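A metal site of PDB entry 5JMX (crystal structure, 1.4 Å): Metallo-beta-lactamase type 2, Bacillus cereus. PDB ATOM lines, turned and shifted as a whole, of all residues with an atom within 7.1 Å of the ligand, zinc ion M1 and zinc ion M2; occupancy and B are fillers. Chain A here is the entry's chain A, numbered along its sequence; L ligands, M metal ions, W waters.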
ATOM      1  N   PRO A  40     -25.481  -5.109  15.792  1.00  0.00           N
ATOM      2  CA  PRO A  40     -24.432  -4.841  14.811  1.00  0.00           C
ATOM      3  C   PRO A  40     -23.071  -5.213  15.359  1.00  0.00           C
ATOM      4  O   PRO A  40     -22.832  -5.172  16.572  1.00  0.00           O
ATOM      5  CB  PRO A  40     -24.520  -3.326  14.624  1.00  0.00           C
ATOM      6  CG  PRO A  40     -24.934  -2.839  15.925  1.00  0.00           C
ATOM      7  CD  PRO A  40     -25.857  -3.889  16.509  1.00  0.00           C
ATOM      8  N   SER A  41     -22.200  -5.564  14.432  1.00  0.00           N
ATOM      9  CA  SER A  41     -20.821  -5.920  14.740  1.00  0.00           C
ATOM     10  C   SER A  41     -19.919  -5.283  13.692  1.00  0.00           C
ATOM     11  O   SER A  41     -20.307  -5.230  12.509  1.00  0.00           O
ATOM     12  CB  SER A  41     -20.674  -7.446  14.675  1.00  0.00           C
ATOM     13  OG  SER A  41     -19.310  -7.840  14.629  1.00  0.00           O
ATOM     14  N   TRP A  59     -21.082 -12.824  11.761  1.00  0.00           N
ATOM     15  CA  TRP A  59     -21.796 -13.693  12.687  1.00  0.00           C
ATOM     16  C   TRP A  59     -21.955 -15.116  12.164  1.00  0.00           C
ATOM     17  O   TRP A  59     -22.041 -16.053  12.953  1.00  0.00           O
ATOM     18  CB  TRP A  59     -23.182 -13.118  12.878  1.00  0.00           C
ATOM     19  CG  TRP A  59     -23.222 -11.764  13.510  1.00  0.00           C
ATOM     20  CD1 TRP A  59     -23.286 -10.553  12.886  1.00  0.00           C
ATOM     21  CD2 TRP A  59     -23.237 -11.487  14.917  1.00  0.00           C
ATOM     22  NE1 TRP A  59     -23.361  -9.534  13.822  1.00  0.00           N
ATOM     23  CE2 TRP A  59     -23.321 -10.085  15.072  1.00  0.00           C
ATOM     24  CE3 TRP A  59     -23.173 -12.285  16.046  1.00  0.00           C
ATOM     25  CZ2 TRP A  59     -23.354  -9.473  16.326  1.00  0.00           C
ATOM     26  CZ3 TRP A  59     -23.207 -11.672  17.290  1.00  0.00           C
ATOM     27  CH2 TRP A  59     -23.285 -10.287  17.413  1.00  0.00           C
ATOM     28  N   HIS A  86     -10.981 -12.721  18.110  1.00  0.00           N
ATOM     29  CA  HIS A  86     -11.242 -13.680  19.182  1.00  0.00           C
ATOM     30  C   HIS A  86     -12.209 -14.724  18.663  1.00  0.00           C
ATOM     31  O   HIS A  86     -12.701 -14.648  17.544  1.00  0.00           O
ATOM     32  CB  HIS A  86     -11.677 -13.043  20.515  1.00  0.00           C
ATOM     33  CG  HIS A  86     -13.050 -12.438  20.538  1.00  0.00           C
ATOM     34  ND1 HIS A  86     -13.263 -11.136  20.105  1.00  0.00           N
ATOM     35  CD2 HIS A  86     -14.212 -12.827  21.120  1.00  0.00           C
ATOM     36  CE1 HIS A  86     -14.528 -10.817  20.304  1.00  0.00           C
ATOM     37  NE2 HIS A  86     -15.139 -11.823  20.906  1.00  0.00           N
ATOM     38  N   ALA A  87     -12.443 -15.756  19.468  1.00  0.00           N
ATOM     39  CA  ALA A  87     -13.193 -16.909  18.997  1.00  0.00           C
ATOM     40  C   ALA A  87     -14.673 -16.891  19.366  1.00  0.00           C
ATOM     41  O   ALA A  87     -15.257 -17.936  19.653  1.00  0.00           O
ATOM     42  CB  ALA A  87     -12.536 -18.184  19.545  1.00  0.00           C
ATOM     43  N   HIS A  88     -15.352 -15.753  19.329  1.00  0.00           N
ATOM     44  CA  HIS A  88     -16.796 -15.709  19.419  1.00  0.00           C
ATOM     45  C   HIS A  88     -17.394 -15.561  18.017  1.00  0.00           C
ATOM     46  O   HIS A  88     -16.722 -15.152  17.084  1.00  0.00           O
ATOM     47  CB  HIS A  88     -17.202 -14.500  20.266  1.00  0.00           C
ATOM     48  CG  HIS A  88     -17.089 -14.684  21.734  1.00  0.00           C
ATOM     49  ND1 HIS A  88     -17.030 -13.626  22.621  1.00  0.00           N
ATOM     50  CD2 HIS A  88     -17.101 -15.806  22.497  1.00  0.00           C
ATOM     51  CE1 HIS A  88     -16.975 -14.096  23.856  1.00  0.00           C
ATOM     52  NE2 HIS A  88     -17.048 -15.413  23.812  1.00  0.00           N
ATOM     53  N   ALA A  89     -18.703 -15.844  17.887  1.00  0.00           N
ATOM     54  CA  ALA A  89     -19.318 -15.986  16.572  1.00  0.00           C
ATOM     55  C   ALA A  89     -19.293 -14.687  15.783  1.00  0.00           C
ATOM     56  O   ALA A  89     -19.196 -14.718  14.565  1.00  0.00           O
ATOM     57  CB  ALA A  89     -20.764 -16.458  16.730  1.00  0.00           C
ATOM     58  N   ASP A  90     -19.403 -13.530  16.440  1.00  0.00           N
ATOM     59  CA  ASP A  90     -19.349 -12.287  15.676  1.00  0.00           C
ATOM     60  C   ASP A  90     -18.019 -12.104  14.955  1.00  0.00           C
ATOM     61  O   ASP A  90     -17.956 -11.399  13.937  1.00  0.00           O
ATOM     62  CB  ASP A  90     -19.712 -11.078  16.563  1.00  0.00           C
ATOM     63  CG  ASP A  90     -18.728 -10.834  17.688  1.00  0.00           C
ATOM     64  OD1 ASP A  90     -18.126 -11.797  18.212  1.00  0.00           O
ATOM     65  OD2 ASP A  90     -18.624  -9.648  18.143  1.00  0.00           O
ATOM     66  N   ARG A  91     -16.954 -12.721  15.438  1.00  0.00           N
ATOM     67  CA  ARG A  91     -15.634 -12.605  14.832  1.00  0.00           C
ATOM     68  C   ARG A  91     -15.354 -13.753  13.881  1.00  0.00           C
ATOM     69  O   ARG A  91     -14.752 -13.537  12.824  1.00  0.00           O
ATOM     70  CB  ARG A  91     -14.540 -12.618  15.925  1.00  0.00           C
ATOM     71  CG  ARG A  91     -14.734 -11.660  17.089  1.00  0.00           C
ATOM     72  CD  ARG A  91     -14.588 -10.233  16.639  1.00  0.00           C
ATOM     73  NE  ARG A  91     -15.848  -9.527  16.689  1.00  0.00           N
ATOM     74  CZ  ARG A  91     -16.051  -8.312  16.188  1.00  0.00           C
ATOM     75  NH1 ARG A  91     -15.089  -7.679  15.550  1.00  0.00           N
ATOM     76  NH2 ARG A  91     -17.216  -7.732  16.356  1.00  0.00           N
ATOM     77  N   HIS A 149     -12.258  -8.894  27.412  1.00  0.00           N
ATOM     78  CA  HIS A 149     -13.559  -9.373  26.995  1.00  0.00           C
ATOM     79  C   HIS A 149     -13.553 -10.888  26.863  1.00  0.00           C
ATOM     80  O   HIS A 149     -14.542 -11.557  27.198  1.00  0.00           O
ATOM     81  CB  HIS A 149     -13.871  -8.737  25.647  1.00  0.00           C
ATOM     82  CG  HIS A 149     -14.986  -9.410  24.910  1.00  0.00           C
ATOM     83  ND1 HIS A 149     -16.288  -9.389  25.347  1.00  0.00           N
ATOM     84  CD2 HIS A 149     -14.983 -10.183  23.795  1.00  0.00           C
ATOM     85  CE1 HIS A 149     -17.050 -10.070  24.523  1.00  0.00           C
ATOM     86  NE2 HIS A 149     -16.276 -10.569  23.566  1.00  0.00           N
ATOM     87  N   THR A 150     -12.448 -11.438  26.357  1.00  0.00           N
ATOM     88  CA  THR A 150     -12.190 -12.860  26.399  1.00  0.00           C
ATOM     89  C   THR A 150     -10.739 -13.089  26.756  1.00  0.00           C
ATOM     90  O   THR A 150      -9.929 -12.160  26.866  1.00  0.00           O
ATOM     91  CB  THR A 150     -12.441 -13.532  25.055  1.00  0.00           C
ATOM     92  OG1 THR A 150     -11.570 -12.903  24.097  1.00  0.00           O
ATOM     93  CG2 THR A 150     -13.888 -13.469  24.674  1.00  0.00           C
ATOM     94  N   GLY A 167     -11.781  -4.114  18.637  1.00  0.00           N
ATOM     95  CA  GLY A 167     -12.562  -5.287  18.767  1.00  0.00           C
ATOM     96  C   GLY A 167     -13.395  -5.208  20.033  1.00  0.00           C
ATOM     97  O   GLY A 167     -13.719  -4.133  20.546  1.00  0.00           O
ATOM     98  N   CYS A 168     -13.765  -6.388  20.526  1.00  0.00           N
ATOM     99  CA  CYS A 168     -14.727  -6.422  21.604  1.00  0.00           C
ATOM    100  C   CYS A 168     -14.104  -6.120  22.942  1.00  0.00           C
ATOM    101  O   CYS A 168     -14.842  -5.940  23.923  1.00  0.00           O
ATOM    102  CB  CYS A 168     -15.519  -7.710  21.545  1.00  0.00           C
ATOM    103  SG  CYS A 168     -16.285  -7.894  19.868  1.00  0.00           S
ATOM    104  N   LEU A 169     -12.763  -5.990  22.999  1.00  0.00           N
ATOM    105  CA  LEU A 169     -12.093  -5.422  24.156  1.00  0.00           C
ATOM    106  C   LEU A 169     -12.507  -3.985  24.420  1.00  0.00           C
ATOM    107  O   LEU A 169     -12.405  -3.519  25.569  1.00  0.00           O
ATOM    108  CB  LEU A 169     -10.581  -5.473  23.924  1.00  0.00           C
ATOM    109  CG  LEU A 169      -9.681  -5.046  25.046  1.00  0.00           C
ATOM    110  CD1 LEU A 169      -9.641  -6.142  26.091  1.00  0.00           C
ATOM    111  CD2 LEU A 169      -8.287  -4.749  24.494  1.00  0.00           C
ATOM    112  N   VAL A 170     -12.954  -3.246  23.414  1.00  0.00           N
ATOM    113  CA  VAL A 170     -13.235  -1.822  23.503  1.00  0.00           C
ATOM    114  C   VAL A 170     -14.728  -1.631  23.295  1.00  0.00           C
ATOM    115  O   VAL A 170     -15.281  -2.053  22.277  1.00  0.00           O
ATOM    116  CB  VAL A 170     -12.405  -1.041  22.468  1.00  0.00           C
ATOM    117  CG1 VAL A 170     -12.738   0.441  22.543  1.00  0.00           C
ATOM    118  CG2 VAL A 170     -10.928  -1.251  22.705  1.00  0.00           C
ATOM    119  N   LYS A 171     -15.380  -0.963  24.253  1.00  0.00           N
ATOM    120  CA  LYS A 171     -16.787  -0.657  24.172  1.00  0.00           C
ATOM    121  C   LYS A 171     -17.007   0.701  23.543  1.00  0.00           C
ATOM    122  O   LYS A 171     -16.230   1.634  23.725  1.00  0.00           O
ATOM    123  CB  LYS A 171     -17.405  -0.654  25.578  1.00  0.00           C
ATOM    124  CG  LYS A 171     -17.123  -1.891  26.397  1.00  0.00           C
ATOM    125  CD  LYS A 171     -17.555  -3.196  25.768  1.00  0.00           C
ATOM    126  CE  LYS A 171     -19.028  -3.303  25.525  1.00  0.00           C
ATOM    127  NZ  LYS A 171     -19.394  -4.745  25.134  1.00  0.00           N
ATOM    128  N   LEU A 178     -20.727  -3.700  30.289  1.00  0.00           N
ATOM    129  CA  LEU A 178     -19.720  -4.479  29.586  1.00  0.00           C
ATOM    130  C   LEU A 178     -20.308  -5.538  28.669  1.00  0.00           C
ATOM    131  O   LEU A 178     -19.543  -6.200  27.970  1.00  0.00           O
ATOM    132  CB  LEU A 178     -18.775  -5.131  30.591  1.00  0.00           C
ATOM    133  CG  LEU A 178     -17.947  -4.151  31.417  1.00  0.00           C
ATOM    134  CD1 LEU A 178     -17.340  -4.873  32.613  1.00  0.00           C
ATOM    135  CD2 LEU A 178     -16.891  -3.478  30.569  1.00  0.00           C
ATOM    136  N   GLY A 179     -21.628  -5.729  28.667  1.00  0.00           N
ATOM    137  CA  GLY A 179     -22.211  -6.773  27.841  1.00  0.00           C
ATOM    138  C   GLY A 179     -22.054  -8.134  28.491  1.00  0.00           C
ATOM    139  O   GLY A 179     -21.959  -8.260  29.713  1.00  0.00           O
ATOM    140  N   ASN A 180     -22.024  -9.178  27.674  1.00  0.00           N
ATOM    141  CA  ASN A 180     -21.919 -10.537  28.205  1.00  0.00           C
ATOM    142  C   ASN A 180     -20.498 -10.775  28.672  1.00  0.00           C
ATOM    143  O   ASN A 180     -19.551 -10.675  27.870  1.00  0.00           O
ATOM    144  CB  ASN A 180     -22.334 -11.543  27.128  1.00  0.00           C
ATOM    145  CG  ASN A 180     -22.406 -12.972  27.646  1.00  0.00           C
ATOM    146  OD1 ASN A 180     -21.562 -13.415  28.418  1.00  0.00           O
ATOM    147  ND2 ASN A 180     -23.451 -13.702  27.245  1.00  0.00           N
ATOM    148  N   VAL A 181     -20.318 -11.057  29.950  1.00  0.00           N
ATOM    149  CA  VAL A 181     -19.009 -11.220  30.566  1.00  0.00           C
ATOM    150  C   VAL A 181     -18.739 -12.686  30.915  1.00  0.00           C
ATOM    151  O   VAL A 181     -17.817 -12.985  31.677  1.00  0.00           O
ATOM    152  CB  VAL A 181     -18.816 -10.281  31.772  1.00  0.00           C
ATOM    153  CG1 VAL A 181     -18.775  -8.825  31.307  1.00  0.00           C
ATOM    154  CG2 VAL A 181     -19.922 -10.512  32.837  1.00  0.00           C
ATOM    155  N   ALA A 182     -19.515 -13.606  30.343  1.00  0.00           N
ATOM    156  CA  ALA A 182     -19.369 -15.017  30.668  1.00  0.00           C
ATOM    157  C   ALA A 182     -17.951 -15.499  30.383  1.00  0.00           C
ATOM    158  O   ALA A 182     -17.398 -16.326  31.110  1.00  0.00           O
ATOM    159  CB  ALA A 182     -20.366 -15.845  29.867  1.00  0.00           C
ATOM    160  N   ASP A 183     -17.349 -15.006  29.308  1.00  0.00           N
ATOM    161  CA  ASP A 183     -16.000 -15.411  28.961  1.00  0.00           C
ATOM    162  C   ASP A 183     -14.956 -14.369  29.317  1.00  0.00           C
ATOM    163  O   ASP A 183     -13.815 -14.474  28.837  1.00  0.00           O
ATOM    164  CB  ASP A 183     -15.926 -15.734  27.468  1.00  0.00           C
ATOM    165  CG  ASP A 183     -16.801 -16.896  27.090  1.00  0.00           C
ATOM    166  OD1 ASP A 183     -17.019 -17.819  27.922  1.00  0.00           O
ATOM    167  OD2 ASP A 183     -17.256 -16.953  25.929  1.00  0.00           O
ATOM    168  N   ALA A 184     -15.286 -13.377  30.145  1.00  0.00           N
ATOM    169  CA  ALA A 184     -14.449 -12.224  30.364  1.00  0.00           C
ATOM    170  C   ALA A 184     -13.641 -12.363  31.642  1.00  0.00           C
ATOM    171  O   ALA A 184     -13.888 -13.233  32.480  1.00  0.00           O
ATOM    172  CB  ALA A 184     -15.307 -10.966  30.430  1.00  0.00           C
ATOM    173  N   TRP A 189      -9.022  -6.987  32.554  1.00  0.00           N
ATOM    174  CA  TRP A 189      -9.412  -6.192  31.381  1.00  0.00           C
ATOM    175  C   TRP A 189      -8.877  -4.772  31.466  1.00  0.00           C
ATOM    176  O   TRP A 189      -8.436  -4.213  30.459  1.00  0.00           O
ATOM    177  CB  TRP A 189     -10.940  -6.237  31.305  1.00  0.00           C
ATOM    178  CG  TRP A 189     -11.599  -5.794  30.048  1.00  0.00           C
ATOM    179  CD1 TRP A 189     -11.101  -4.971  29.041  1.00  0.00           C
ATOM    180  CD2 TRP A 189     -12.927  -6.136  29.663  1.00  0.00           C
ATOM    181  NE1 TRP A 189     -12.078  -4.781  28.091  1.00  0.00           N
ATOM    182  CE2 TRP A 189     -13.183  -5.512  28.423  1.00  0.00           C
ATOM    183  CE3 TRP A 189     -13.901  -6.947  30.227  1.00  0.00           C
ATOM    184  CZ2 TRP A 189     -14.420  -5.650  27.772  1.00  0.00           C
ATOM    185  CZ3 TRP A 189     -15.118  -7.081  29.606  1.00  0.00           C
ATOM    186  CH2 TRP A 189     -15.365  -6.453  28.356  1.00  0.00           C
ATOM    187  N   GLY A 209     -15.722  -3.215  18.740  1.00  0.00           N
ATOM    188  CA  GLY A 209     -16.337  -4.390  18.195  1.00  0.00           C
ATOM    189  C   GLY A 209     -17.782  -4.176  17.786  1.00  0.00           C
ATOM    190  O   GLY A 209     -18.262  -4.812  16.840  1.00  0.00           O
ATOM    191  N   HIS A 210     -18.502  -3.308  18.501  1.00  0.00           N
ATOM    192  CA  HIS A 210     -19.892  -2.982  18.241  1.00  0.00           C
ATOM    193  C   HIS A 210     -20.051  -1.488  18.505  1.00  0.00           C
ATOM    194  O   HIS A 210     -19.534  -0.993  19.509  1.00  0.00           O
ATOM    195  CB  HIS A 210     -20.828  -3.791  19.186  1.00  0.00           C
ATOM    196  CG  HIS A 210     -20.503  -5.254  19.223  1.00  0.00           C
ATOM    197  ND1 HIS A 210     -21.098  -6.171  18.367  1.00  0.00           N
ATOM    198  CD2 HIS A 210     -19.581  -5.951  19.933  1.00  0.00           C
ATOM    199  CE1 HIS A 210     -20.580  -7.370  18.592  1.00  0.00           C
ATOM    200  NE2 HIS A 210     -19.642  -7.264  19.517  1.00  0.00           N
HETATM  201  O1  LIG L   1     -18.653  -7.995  22.100  1.00  0.00           O
HETATM  202  C1  LIG L   1     -19.455  -8.664  22.813  1.00  0.00           C
HETATM  203  O2  LIG L   1     -20.068  -8.143  23.789  1.00  0.00           O
HETATM  204  C2  LIG L   1     -19.555 -10.177  22.603  1.00  0.00           C
HETATM  205  C3  LIG L   1     -20.162 -10.958  23.554  1.00  0.00           C
HETATM  206  C4  LIG L   1     -20.260 -12.420  23.609  1.00  0.00           C
HETATM  207  C5  LIG L   1     -20.619 -13.281  22.552  1.00  0.00           C
HETATM  208  C6  LIG L   1     -20.682 -14.663  22.693  1.00  0.00           C
HETATM  209  C7  LIG L   1     -20.385 -15.191  23.960  1.00  0.00           C
HETATM  210  F1  LIG L   1     -20.432 -16.560  24.131  1.00  0.00           F
HETATM  211  C8  LIG L   1     -20.028 -14.448  25.026  1.00  0.00           C
HETATM  212  C9  LIG L   1     -19.975 -13.066  24.846  1.00  0.00           C
HETATM  213  S1  LIG L   1     -18.859 -10.863  21.170  1.00  0.00           S
HETATM  214 ZN    ZN M   1     -16.871 -11.679  21.992  1.00  0.00          ZN
HETATM  215 ZN    ZN M   2     -18.352  -8.809  20.082  1.00  0.00          ZN
HETATM  216  O   HOH W   1     -20.396 -13.153  19.147  1.00  0.00           O
HETATM  217  O   HOH W   2     -17.656  -5.709  23.239  1.00  0.00           O
HETATM  218  O   HOH W   3     -22.422  -8.774  24.974  1.00  0.00           O
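Zinc ion M2 is bound by a ring nitrogen (NE2) of His 210 (2.1 Å), the side-chain carboxylate (OD2) of Asp 90 (2.1 Å), an oxygen (O1) of the ligand (2.2 Å), the side-chain sulfur (SG) of Cys 168 (2.3 Å) and a sulfur (S1) of the ligand (2.4 Å).
The nearest printed residue that does not touch zinc ion M2 is Arg 91 (4.04 Å).
The side-chain sulfur (SG) of Cys 168 sits close to the guanidinium group (NE) of Arg 91 (3.6 Å). O of Leu 178 sits at hydrogen-bond distance from NZ of Lys 171 (3.2 Å). The side-chain amide oxygen (OD1) of Asn 180 is in hydrogen-bond range of the backbone NH (N) of Ala 182 (2.8 Å). A ring nitrogen (ND1) of His 210 is in hydrogen-bond range of the backbone carbonyl oxygen (O) of Pro 40, at 2.7 Å. A ring nitrogen (NE2) of His 88 lies within hydrogen-bond range of the side-chain carboxylate (OD2) of Asp 183 (2.6 Å). The guanidinium group (NE) of Arg 91 is in salt-bridge range of the side-chain carboxylate (OD1) of Asp 90 (3.6 Å).
Zinc ion M1 is bound by NE2 of His 149, NE2 of His 86, ND1 of His 88 and S1 of the ligand.
O2 of the ligand is in salt-bridge range of NZ of Lys 171.
Water W3 lies within hydrogen-bond range of an oxygen (O2) of the ligand (2.7 Å) and the backbone NH of Asn 180 (2.8 Å). Water W2 lies within hydrogen-bond range of NZ of Lys 171, O of Cys 168 and O2 of the ligand. Water W1 lies within hydrogen-bond range of OD1 of Asp 90 and N of Ala 89.
CB of Asn 180 touches C9 of the ligand, at 3.6 Å. OD2 of Asp 183 touches F1 of the ligand (3.7 Å). Of the 26 residues printed, 9 come within 4 Å of the ligand.
Of the 26 residues printed, 4 come within 4 Å of zinc ion M1. The nearest printed residue that does not touch zinc ion M1 is Cys 168 (4.2 Å).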
